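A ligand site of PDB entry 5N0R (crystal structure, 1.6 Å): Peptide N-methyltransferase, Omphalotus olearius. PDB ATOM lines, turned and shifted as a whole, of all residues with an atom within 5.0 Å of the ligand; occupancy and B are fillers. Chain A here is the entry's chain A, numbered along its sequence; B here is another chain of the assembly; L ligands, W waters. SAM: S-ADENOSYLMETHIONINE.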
ATOM      1  N   ILE A  18     -28.312  12.679  20.619  1.00  0.00           N
ATOM      2  CA  ILE A  18     -26.851  12.876  20.542  1.00  0.00           C
ATOM      3  C   ILE A  18     -26.492  14.368  20.520  1.00  0.00           C
ATOM      4  O   ILE A  18     -25.614  14.814  21.287  1.00  0.00           O
ATOM      5  CB  ILE A  18     -26.264  12.143  19.308  1.00  0.00           C
ATOM      6  CG1 ILE A  18     -26.490  10.622  19.431  1.00  0.00           C
ATOM      7  CG2 ILE A  18     -24.790  12.457  19.116  1.00  0.00           C
ATOM      8  CD1 ILE A  18     -25.810   9.949  20.608  1.00  0.00           C
ATOM      9  N   ILE A  43     -23.047  13.414  28.203  1.00  0.00           N
ATOM     10  CA  ILE A  43     -21.641  13.758  27.952  1.00  0.00           C
ATOM     11  C   ILE A  43     -21.399  15.136  27.331  1.00  0.00           C
ATOM     12  O   ILE A  43     -20.292  15.361  26.803  1.00  0.00           O
ATOM     13  CB  ILE A  43     -20.913  12.647  27.155  1.00  0.00           C
ATOM     14  CG1 ILE A  43     -21.527  12.441  25.788  1.00  0.00           C
ATOM     15  CG2 ILE A  43     -20.992  11.350  27.932  1.00  0.00           C
ATOM     16  CD1 ILE A  43     -20.772  11.438  24.939  1.00  0.00           C
ATOM     17  N   TYR A  97     -27.695   9.450  27.510  1.00  0.00           N
ATOM     18  CA  TYR A  97     -27.553  10.092  26.201  1.00  0.00           C
ATOM     19  C   TYR A  97     -27.878   9.126  25.053  1.00  0.00           C
ATOM     20  O   TYR A  97     -27.731   7.902  25.163  1.00  0.00           O
ATOM     21  CB  TYR A  97     -26.215  10.788  26.050  1.00  0.00           C
ATOM     22  CG  TYR A  97     -25.063   9.925  25.728  1.00  0.00           C
ATOM     23  CD1 TYR A  97     -24.322   9.313  26.728  1.00  0.00           C
ATOM     24  CD2 TYR A  97     -24.664   9.742  24.398  1.00  0.00           C
ATOM     25  CE1 TYR A  97     -23.233   8.508  26.418  1.00  0.00           C
ATOM     26  CE2 TYR A  97     -23.580   8.938  24.080  1.00  0.00           C
ATOM     27  CZ  TYR A  97     -22.866   8.318  25.096  1.00  0.00           C
ATOM     28  OH  TYR A  97     -21.768   7.526  24.795  1.00  0.00           O
ATOM     29  N   GLY A  98     -28.330   9.718  23.958  1.00  0.00           N
ATOM     30  CA  GLY A  98     -28.783   8.963  22.788  1.00  0.00           C
ATOM     31  C   GLY A  98     -30.121   8.276  23.024  1.00  0.00           C
ATOM     32  O   GLY A  98     -31.069   8.892  23.507  1.00  0.00           O
ATOM     33  N   HIS A  99     -30.183   6.986  22.649  1.00  0.00           N
ATOM     34  CA  HIS A  99     -31.283   6.064  23.000  1.00  0.00           C
ATOM     35  C   HIS A  99     -30.801   5.317  24.261  1.00  0.00           C
ATOM     36  O   HIS A  99     -29.690   4.741  24.242  1.00  0.00           O
ATOM     37  CB  HIS A  99     -31.494   5.078  21.835  1.00  0.00           C
ATOM     38  CG  HIS A  99     -32.634   4.109  21.978  1.00  0.00           C
ATOM     39  ND1 HIS A  99     -32.835   3.294  23.076  1.00  0.00           N
ATOM     40  CD2 HIS A  99     -33.591   3.765  21.083  1.00  0.00           C
ATOM     41  CE1 HIS A  99     -33.874   2.509  22.863  1.00  0.00           C
ATOM     42  NE2 HIS A  99     -34.353   2.769  21.648  1.00  0.00           N
ATOM     43  N   VAL A 102     -29.614   1.482  23.756  1.00  0.00           N
ATOM     44  CA  VAL A 102     -28.718   1.144  22.646  1.00  0.00           C
ATOM     45  C   VAL A 102     -27.293   1.264  23.159  1.00  0.00           C
ATOM     46  O   VAL A 102     -26.809   2.364  23.426  1.00  0.00           O
ATOM     47  CB  VAL A 102     -29.017   2.067  21.432  1.00  0.00           C
ATOM     48  CG1 VAL A 102     -27.974   1.978  20.330  1.00  0.00           C
ATOM     49  CG2 VAL A 102     -30.403   1.732  20.855  1.00  0.00           C
ATOM     50  N   PHE A 103     -26.630   0.116  23.313  1.00  0.00           N
ATOM     51  CA  PHE A 103     -25.290   0.033  23.892  1.00  0.00           C
ATOM     52  C   PHE A 103     -25.243   0.658  25.310  1.00  0.00           C
ATOM     53  O   PHE A 103     -24.356   1.460  25.612  1.00  0.00           O
ATOM     54  CB  PHE A 103     -24.230   0.635  22.950  1.00  0.00           C
ATOM     55  CG  PHE A 103     -24.043  -0.137  21.660  1.00  0.00           C
ATOM     56  CD1 PHE A 103     -24.993  -0.064  20.645  1.00  0.00           C
ATOM     57  CD2 PHE A 103     -22.908  -0.913  21.444  1.00  0.00           C
ATOM     58  CE1 PHE A 103     -24.845  -0.787  19.471  1.00  0.00           C
ATOM     59  CE2 PHE A 103     -22.760  -1.636  20.270  1.00  0.00           C
ATOM     60  CZ  PHE A 103     -23.727  -1.558  19.279  1.00  0.00           C
ATOM     61  N   VAL A 104     -26.193   0.282  26.160  1.00  0.00           N
ATOM     62  CA  VAL A 104     -26.254   0.751  27.569  1.00  0.00           C
ATOM     63  C   VAL A 104     -26.585  -0.438  28.501  1.00  0.00           C
ATOM     64  O   VAL A 104     -27.620  -1.071  28.328  1.00  0.00           O
ATOM     65  CB  VAL A 104     -27.330   1.847  27.775  1.00  0.00           C
ATOM     66  CG1 VAL A 104     -27.340   2.363  29.217  1.00  0.00           C
ATOM     67  CG2 VAL A 104     -27.134   3.017  26.821  1.00  0.00           C
ATOM     68  N   VAL A 127     -33.156   9.076  20.004  1.00  0.00           N
ATOM     69  CA  VAL A 127     -32.314   9.126  18.798  1.00  0.00           C
ATOM     70  C   VAL A 127     -30.903   8.605  19.119  1.00  0.00           C
ATOM     71  O   VAL A 127     -30.195   9.216  19.923  1.00  0.00           O
ATOM     72  CB  VAL A 127     -32.253  10.571  18.233  1.00  0.00           C
ATOM     73  CG1 VAL A 127     -31.239  10.706  17.106  1.00  0.00           C
ATOM     74  CG2 VAL A 127     -33.643  11.041  17.808  1.00  0.00           C
ATOM     75  N   SER A 128     -30.506   7.498  18.515  1.00  0.00           N
ATOM     76  CA  SER A 128     -29.163   6.902  18.715  1.00  0.00           C
ATOM     77  C   SER A 128     -28.057   7.451  17.808  1.00  0.00           C
ATOM     78  O   SER A 128     -28.301   8.156  16.820  1.00  0.00           O
ATOM     79  CB  SER A 128     -29.235   5.387  18.510  1.00  0.00           C
ATOM     80  OG  SER A 128     -29.245   5.073  17.107  1.00  0.00           O
ATOM     81  N   ALA A 129     -26.807   7.105  18.124  1.00  0.00           N
ATOM     82  CA  ALA A 129     -25.690   7.426  17.230  1.00  0.00           C
ATOM     83  C   ALA A 129     -25.833   6.803  15.838  1.00  0.00           C
ATOM     84  O   ALA A 129     -25.372   7.400  14.844  1.00  0.00           O
ATOM     85  CB  ALA A 129     -24.362   7.020  17.848  1.00  0.00           C
ATOM     86  N   GLU A 130     -26.462   5.634  15.754  1.00  0.00           N
ATOM     87  CA  GLU A 130     -26.706   4.993  14.450  1.00  0.00           C
ATOM     88  C   GLU A 130     -27.782   5.770  13.654  1.00  0.00           C
ATOM     89  O   GLU A 130     -27.646   5.943  12.421  1.00  0.00           O
ATOM     90  CB  GLU A 130     -27.102   3.514  14.618  1.00  0.00           C
ATOM     91  CG  GLU A 130     -27.342   2.806  13.280  1.00  0.00           C
ATOM     92  CD  GLU A 130     -27.433   1.303  13.377  1.00  0.00           C
ATOM     93  OE1 GLU A 130     -28.548   0.773  13.559  1.00  0.00           O
ATOM     94  OE2 GLU A 130     -26.385   0.644  13.233  1.00  0.00           O
ATOM     95  N   LEU A 169     -19.935  -0.410  13.254  1.00  0.00           N
ATOM     96  CA  LEU A 169     -19.200  -0.848  14.448  1.00  0.00           C
ATOM     97  C   LEU A 169     -19.111   0.288  15.495  1.00  0.00           C
ATOM     98  O   LEU A 169     -18.520   1.325  15.216  1.00  0.00           O
ATOM     99  CB  LEU A 169     -17.783  -1.324  14.086  1.00  0.00           C
ATOM    100  CG  LEU A 169     -17.662  -2.493  13.102  1.00  0.00           C
ATOM    101  CD1 LEU A 169     -16.189  -2.800  12.796  1.00  0.00           C
ATOM    102  CD2 LEU A 169     -18.328  -3.737  13.656  1.00  0.00           C
ATOM    103  N   PHE A 170     -19.716   0.057  16.667  1.00  0.00           N
ATOM    104  CA  PHE A 170     -19.634   0.972  17.823  1.00  0.00           C
ATOM    105  C   PHE A 170     -18.378   0.640  18.677  1.00  0.00           C
ATOM    106  O   PHE A 170     -17.884  -0.488  18.632  1.00  0.00           O
ATOM    107  CB  PHE A 170     -20.853   0.800  18.755  1.00  0.00           C
ATOM    108  CG  PHE A 170     -22.140   1.506  18.316  1.00  0.00           C
ATOM    109  CD1 PHE A 170     -22.817   1.132  17.149  1.00  0.00           C
ATOM    110  CD2 PHE A 170     -22.735   2.455  19.138  1.00  0.00           C
ATOM    111  CE1 PHE A 170     -24.006   1.759  16.781  1.00  0.00           C
ATOM    112  CE2 PHE A 170     -23.941   3.087  18.793  1.00  0.00           C
ATOM    113  CZ  PHE A 170     -24.565   2.736  17.606  1.00  0.00           C
ATOM    114  N   GLN A 171     -17.899   1.610  19.448  1.00  0.00           N
ATOM    115  CA  GLN A 171     -16.812   1.410  20.442  1.00  0.00           C
ATOM    116  C   GLN A 171     -15.483   0.954  19.827  1.00  0.00           C
ATOM    117  O   GLN A 171     -14.720   0.166  20.442  1.00  0.00           O
ATOM    118  CB  GLN A 171     -17.291   0.502  21.602  1.00  0.00           C
ATOM    119  CG  GLN A 171     -18.573   1.034  22.231  1.00  0.00           C
ATOM    120  CD  GLN A 171     -18.936   0.520  23.605  1.00  0.00           C
ATOM    121  OE1 GLN A 171     -19.701   1.186  24.310  1.00  0.00           O
ATOM    122  NE2 GLN A 171     -18.419  -0.638  23.998  1.00  0.00           N
ATOM    123  N   VAL A 172     -15.179   1.496  18.651  1.00  0.00           N
ATOM    124  CA  VAL A 172     -13.916   1.228  17.947  1.00  0.00           C
ATOM    125  C   VAL A 172     -12.717   1.915  18.607  1.00  0.00           C
ATOM    126  O   VAL A 172     -11.570   1.584  18.296  1.00  0.00           O
ATOM    127  CB  VAL A 172     -13.985   1.557  16.435  1.00  0.00           C
ATOM    128  CG1 VAL A 172     -14.986   0.648  15.738  1.00  0.00           C
ATOM    129  CG2 VAL A 172     -14.308   3.022  16.159  1.00  0.00           C
ATOM    130  N   TYR A 210     -16.777   8.102  11.664  1.00  0.00           N
ATOM    131  CA  TYR A 210     -17.942   8.952  11.921  1.00  0.00           C
ATOM    132  C   TYR A 210     -18.014   9.432  13.375  1.00  0.00           C
ATOM    133  O   TYR A 210     -17.983   8.623  14.309  1.00  0.00           O
ATOM    134  CB  TYR A 210     -19.229   8.208  11.564  1.00  0.00           C
ATOM    135  CG  TYR A 210     -20.488   9.022  11.853  1.00  0.00           C
ATOM    136  CD1 TYR A 210     -20.746  10.206  11.175  1.00  0.00           C
ATOM    137  CD2 TYR A 210     -21.400   8.619  12.832  1.00  0.00           C
ATOM    138  CE1 TYR A 210     -21.880  10.969  11.448  1.00  0.00           C
ATOM    139  CE2 TYR A 210     -22.539   9.362  13.118  1.00  0.00           C
ATOM    140  CZ  TYR A 210     -22.770  10.539  12.432  1.00  0.00           C
ATOM    141  OH  TYR A 210     -23.901  11.287  12.714  1.00  0.00           O
ATOM    142  N   ILE A 211     -18.122  10.756  13.541  1.00  0.00           N
ATOM    143  CA  ILE A 211     -18.470  11.377  14.832  1.00  0.00           C
ATOM    144  C   ILE A 211     -19.590  12.406  14.578  1.00  0.00           C
ATOM    145  O   ILE A 211     -19.376  13.434  13.907  1.00  0.00           O
ATOM    146  CB  ILE A 211     -17.273  12.059  15.554  1.00  0.00           C
ATOM    147  CG1 ILE A 211     -16.061  11.100  15.673  1.00  0.00           C
ATOM    148  CG2 ILE A 211     -17.710  12.565  16.925  1.00  0.00           C
ATOM    149  CD1 ILE A 211     -14.785  11.763  16.147  1.00  0.00           C
ATOM    150  N   ALA A 212     -20.778  12.113  15.090  1.00  0.00           N
ATOM    151  CA  ALA A 212     -21.908  13.055  15.047  1.00  0.00           C
ATOM    152  C   ALA A 212     -21.560  14.325  15.833  1.00  0.00           C
ATOM    153  O   ALA A 212     -20.943  14.253  16.911  1.00  0.00           O
ATOM    154  CB  ALA A 212     -23.150  12.413  15.634  1.00  0.00           C
ATOM    155  N   MET A 214     -21.920  17.115  18.404  1.00  0.00           N
ATOM    156  CA  MET A 214     -22.568  17.145  19.722  1.00  0.00           C
ATOM    157  C   MET A 214     -23.087  18.537  20.093  1.00  0.00           C
ATOM    158  O   MET A 214     -24.017  18.641  20.883  1.00  0.00           O
ATOM    159  CB  MET A 214     -21.628  16.553  20.787  1.00  0.00           C
ATOM    160  CG  MET A 214     -21.470  15.042  20.612  1.00  0.00           C
ATOM    161  SD  MET A 214     -20.120  14.262  21.528  1.00  0.00           S
ATOM    162  CE  MET A 214     -20.607  14.859  23.149  1.00  0.00           C
ATOM    163  N   GLY A 241     -13.419   7.893  22.070  1.00  0.00           N
ATOM    164  CA  GLY A 241     -14.564   7.327  22.784  1.00  0.00           C
ATOM    165  C   GLY A 241     -15.948   7.602  22.210  1.00  0.00           C
ATOM    166  O   GLY A 241     -16.920   6.956  22.620  1.00  0.00           O
ATOM    167  N   VAL A 242     -16.067   8.571  21.305  1.00  0.00           N
ATOM    168  CA  VAL A 242     -17.344   8.810  20.609  1.00  0.00           C
ATOM    169  C   VAL A 242     -17.249   8.498  19.101  1.00  0.00           C
ATOM    170  O   VAL A 242     -18.056   8.979  18.320  1.00  0.00           O
ATOM    171  CB  VAL A 242     -17.899  10.235  20.864  1.00  0.00           C
ATOM    172  CG1 VAL A 242     -18.391  10.363  22.295  1.00  0.00           C
ATOM    173  CG2 VAL A 242     -16.883  11.330  20.518  1.00  0.00           C
ATOM    174  N   SER A 243     -16.273   7.659  18.717  1.00  0.00           N
ATOM    175  CA  SER A 243     -16.073   7.274  17.300  1.00  0.00           C
ATOM    176  C   SER A 243     -16.839   5.999  16.954  1.00  0.00           C
ATOM    177  O   SER A 243     -16.848   5.028  17.750  1.00  0.00           O
ATOM    178  CB  SER A 243     -14.580   7.029  17.012  1.00  0.00           C
ATOM    179  OG  SER A 243     -13.831   8.229  17.131  1.00  0.00           O
ATOM    180  N   THR A 244     -17.451   6.001  15.769  1.00  0.00           N
ATOM    181  CA  THR A 244     -18.130   4.837  15.188  1.00  0.00           C
ATOM    182  C   THR A 244     -17.568   4.628  13.773  1.00  0.00           C
ATOM    183  O   THR A 244     -17.235   5.605  13.102  1.00  0.00           O
ATOM    184  CB  THR A 244     -19.660   5.090  15.176  1.00  0.00           C
ATOM    185  OG1 THR A 244     -20.148   5.149  16.524  1.00  0.00           O
ATOM    186  CG2 THR A 244     -20.443   4.018  14.411  1.00  0.00           C
ATOM    187  N   GLY B 404     -17.853   8.845  27.603  1.00  0.00           N
ATOM    188  CA  GLY B 404     -19.220   8.563  28.029  1.00  0.00           C
ATOM    189  C   GLY B 404     -19.481   7.086  28.098  1.00  0.00           C
ATOM    190  O   GLY B 404     -20.345   6.558  27.394  1.00  0.00           O
ATOM    191  N   MVA B 405     -18.708   6.418  28.937  1.00  0.00           N
ATOM    192  CN  MVA B 405     -17.522   6.990  29.544  1.00  0.00           C
ATOM    193  CA  MVA B 405     -18.975   5.043  29.226  1.00  0.00           C
ATOM    194  CB  MVA B 405     -20.398   4.804  29.682  1.00  0.00           C
ATOM    195  CG1 MVA B 405     -20.390   3.462  30.385  1.00  0.00           C
ATOM    196  CG2 MVA B 405     -21.370   4.739  28.520  1.00  0.00           C
ATOM    197  C   MVA B 405     -18.806   4.134  28.063  1.00  0.00           C
ATOM    198  O   MVA B 405     -18.933   4.560  26.915  1.00  0.00           O
ATOM    199  N   ILE B 406     -18.541   2.880  28.368  1.00  0.00           N
ATOM    200  CA  ILE B 406     -18.495   1.824  27.399  1.00  0.00           C
ATOM    201  C   ILE B 406     -19.427   0.689  27.793  1.00  0.00           C
ATOM    202  O   ILE B 406     -19.491   0.308  28.953  1.00  0.00           O
ATOM    203  CB  ILE B 406     -17.091   1.271  27.300  1.00  0.00           C
ATOM    204  CG1 ILE B 406     -16.345   2.038  26.236  1.00  0.00           C
ATOM    205  CG2 ILE B 406     -17.112  -0.197  26.912  1.00  0.00           C
ATOM    206  CD1 ILE B 406     -15.690   1.079  25.314  1.00  0.00           C
ATOM    207  N   GLY B 407     -20.164   0.160  26.827  1.00  0.00           N
ATOM    208  CA  GLY B 407     -20.982  -1.013  27.057  1.00  0.00           C
ATOM    209  C   GLY B 407     -20.132  -2.260  27.100  1.00  0.00           C
ATOM    210  O   GLY B 407     -19.159  -2.381  26.341  1.00  0.00           O
HETATM  211  N   SAM L   1     -26.722   5.134  23.899  1.00  0.00           N
HETATM  212  CA  SAM L   1     -25.780   5.631  22.902  1.00  0.00           C
HETATM  213  C   SAM L   1     -26.525   5.784  21.582  1.00  0.00           C
HETATM  214  O   SAM L   1     -25.862   5.946  20.520  1.00  0.00           O
HETATM  215  OXT SAM L   1     -27.782   5.763  21.597  1.00  0.00           O
HETATM  216  CB  SAM L   1     -24.507   4.743  22.738  1.00  0.00           C
HETATM  217  CG  SAM L   1     -23.690   4.492  24.034  1.00  0.00           C
HETATM  218  SD  SAM L   1     -22.244   3.586  23.886  1.00  0.00           S
HETATM  219  CE  SAM L   1     -21.816   3.151  25.438  1.00  0.00           C
HETATM  220  C5' SAM L   1     -20.953   4.506  23.266  1.00  0.00           C
HETATM  221  C4' SAM L   1     -20.662   4.394  21.764  1.00  0.00           C
HETATM  222  O4' SAM L   1     -21.662   5.119  21.008  1.00  0.00           O
HETATM  223  C3' SAM L   1     -19.373   5.042  21.267  1.00  0.00           C
HETATM  224  O3' SAM L   1     -18.168   4.260  21.437  1.00  0.00           O
HETATM  225  C2' SAM L   1     -19.661   5.279  19.803  1.00  0.00           C
HETATM  226  O2' SAM L   1     -19.517   4.083  19.041  1.00  0.00           O
HETATM  227  C1' SAM L   1     -21.129   5.700  19.831  1.00  0.00           C
HETATM  228  N9  SAM L   1     -21.244   7.184  19.902  1.00  0.00           N
HETATM  229  C8  SAM L   1     -21.489   7.963  20.978  1.00  0.00           C
HETATM  230  N7  SAM L   1     -21.506   9.280  20.640  1.00  0.00           N
HETATM  231  C5  SAM L   1     -21.241   9.340  19.320  1.00  0.00           C
HETATM  232  C6  SAM L   1     -21.092  10.403  18.335  1.00  0.00           C
HETATM  233  N6  SAM L   1     -21.231  11.698  18.722  1.00  0.00           N
HETATM  234  N1  SAM L   1     -20.818  10.048  17.066  1.00  0.00           N
HETATM  235  C2  SAM L   1     -20.679   8.754  16.679  1.00  0.00           C
HETATM  236  N3  SAM L   1     -20.786   7.728  17.544  1.00  0.00           N
HETATM  237  C4  SAM L   1     -21.069   7.970  18.842  1.00  0.00           C
HETATM  238  O   HOH W   1     -22.175  11.801  21.649  1.00  0.00           O
HETATM  239  O   HOH W   2     -25.955   6.282  26.439  1.00  0.00           O
HETATM  240  O   HOH W   3     -15.461   4.495  20.032  1.00  0.00           O
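The backbone carbonyl oxygen of Thr 244 sits at hydrogen-bond distance from the backbone NH of Tyr 210. N of Gly 407 of chain B sits at hydrogen-bond distance from OE1 of Gln 171 (2.8 Å). The side-chain hydroxyl (OH) of Tyr 97 sits at hydrogen-bond distance from the backbone carbonyl oxygen (O) of Gly 404 of chain B (3.1 Å). The side-chain hydroxyl (OG) of Ser 128 is in hydrogen-bond range of the backbone NH (N) of Glu 130, 3.1 Å away.
OG1 of Thr 244 is in hydrogen-bond range of O2' of the ligand (2.8 Å). O of Val 102 sits at hydrogen-bond distance from N of the ligand. The backbone NH (N) of Ala 129 sits at hydrogen-bond distance from an oxygen (O) of the ligand (2.8 Å). A nitrogen (N1) of the ligand lies within hydrogen-bond range of the backbone NH of Ala 212, at 2.9 Å. The backbone carbonyl oxygen (O) of Ala 212 lies within hydrogen-bond range of a nitrogen (N6) of the ligand, 3.1 Å away. An oxygen (OXT) of the ligand sits at hydrogen-bond distance from the backbone NH of His 99 (2.9 Å). The backbone carbonyl oxygen (O) of His 99 lies within hydrogen-bond range of a nitrogen (N) of the ligand (3.0 Å). The backbone NH (N) of Gln 171 sits at hydrogen-bond distance from an oxygen (O2') of the ligand. O of Ser 243 is in hydrogen-bond range of O2' of the ligand. O of Gly 241 sits at hydrogen-bond distance from O3' of the ligand (3.2 Å). O of Tyr 97 is in hydrogen-bond range of N of the ligand (3.2 Å).
Water W1 bridges N7 of the ligand (2.8 Å) and SD of Met 214 (3.2 Å). Water W2 bridges the backbone carbonyl oxygen of Tyr 97 (2.7 Å) and a nitrogen (N) of the ligand (2.9 Å). Water W3 lies within hydrogen-bond range of the backbone carbonyl oxygen (O) of Ser 243, an oxygen (O3') of the ligand and the backbone NH (N) of Val 172.
The backbone carbonyl oxygen (O) of Phe 103 lies close to a sulfur (SD) of the ligand (3.5 Å). N3 of the ligand lies close to O of Val 242, at 3.1 Å. CG2 of Ile 18 touches N6 of the ligand, 3.7 Å away. Gly 98 touches the ligand. Val 104 touches the ligand. Ser 128 touches the ligand. Phe 170 touches the ligand (CA to O2', 3.3 Å). O of Tyr 210 touches C2 of the ligand (3.6 Å). Ile 211 touches the ligand. Met 214 touches the ligand (CG to N6, 3.8 Å). MVA 405 of chain B touches the ligand (CG2 to CE, 3.5 Å). Gly 407 of chain B touches the ligand (N to CE, 3.7 Å). 21 residues have an atom within 4 Å of the ligand: Ile 18, Tyr 97, Gly 98, His 99, Val 102, Phe 103, Val 104, Ser 128, Ala 129, Phe 170, Gln 171, Tyr 210, Ile 211, Ala 212, Met 214, Gly 241, Val 242, Ser 243, Thr 244, MVA 405 of chain B and Gly 407 of chain B. The nearest printed residue that does not touch the ligand is Ile 406 of chain B (4.1 Å).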
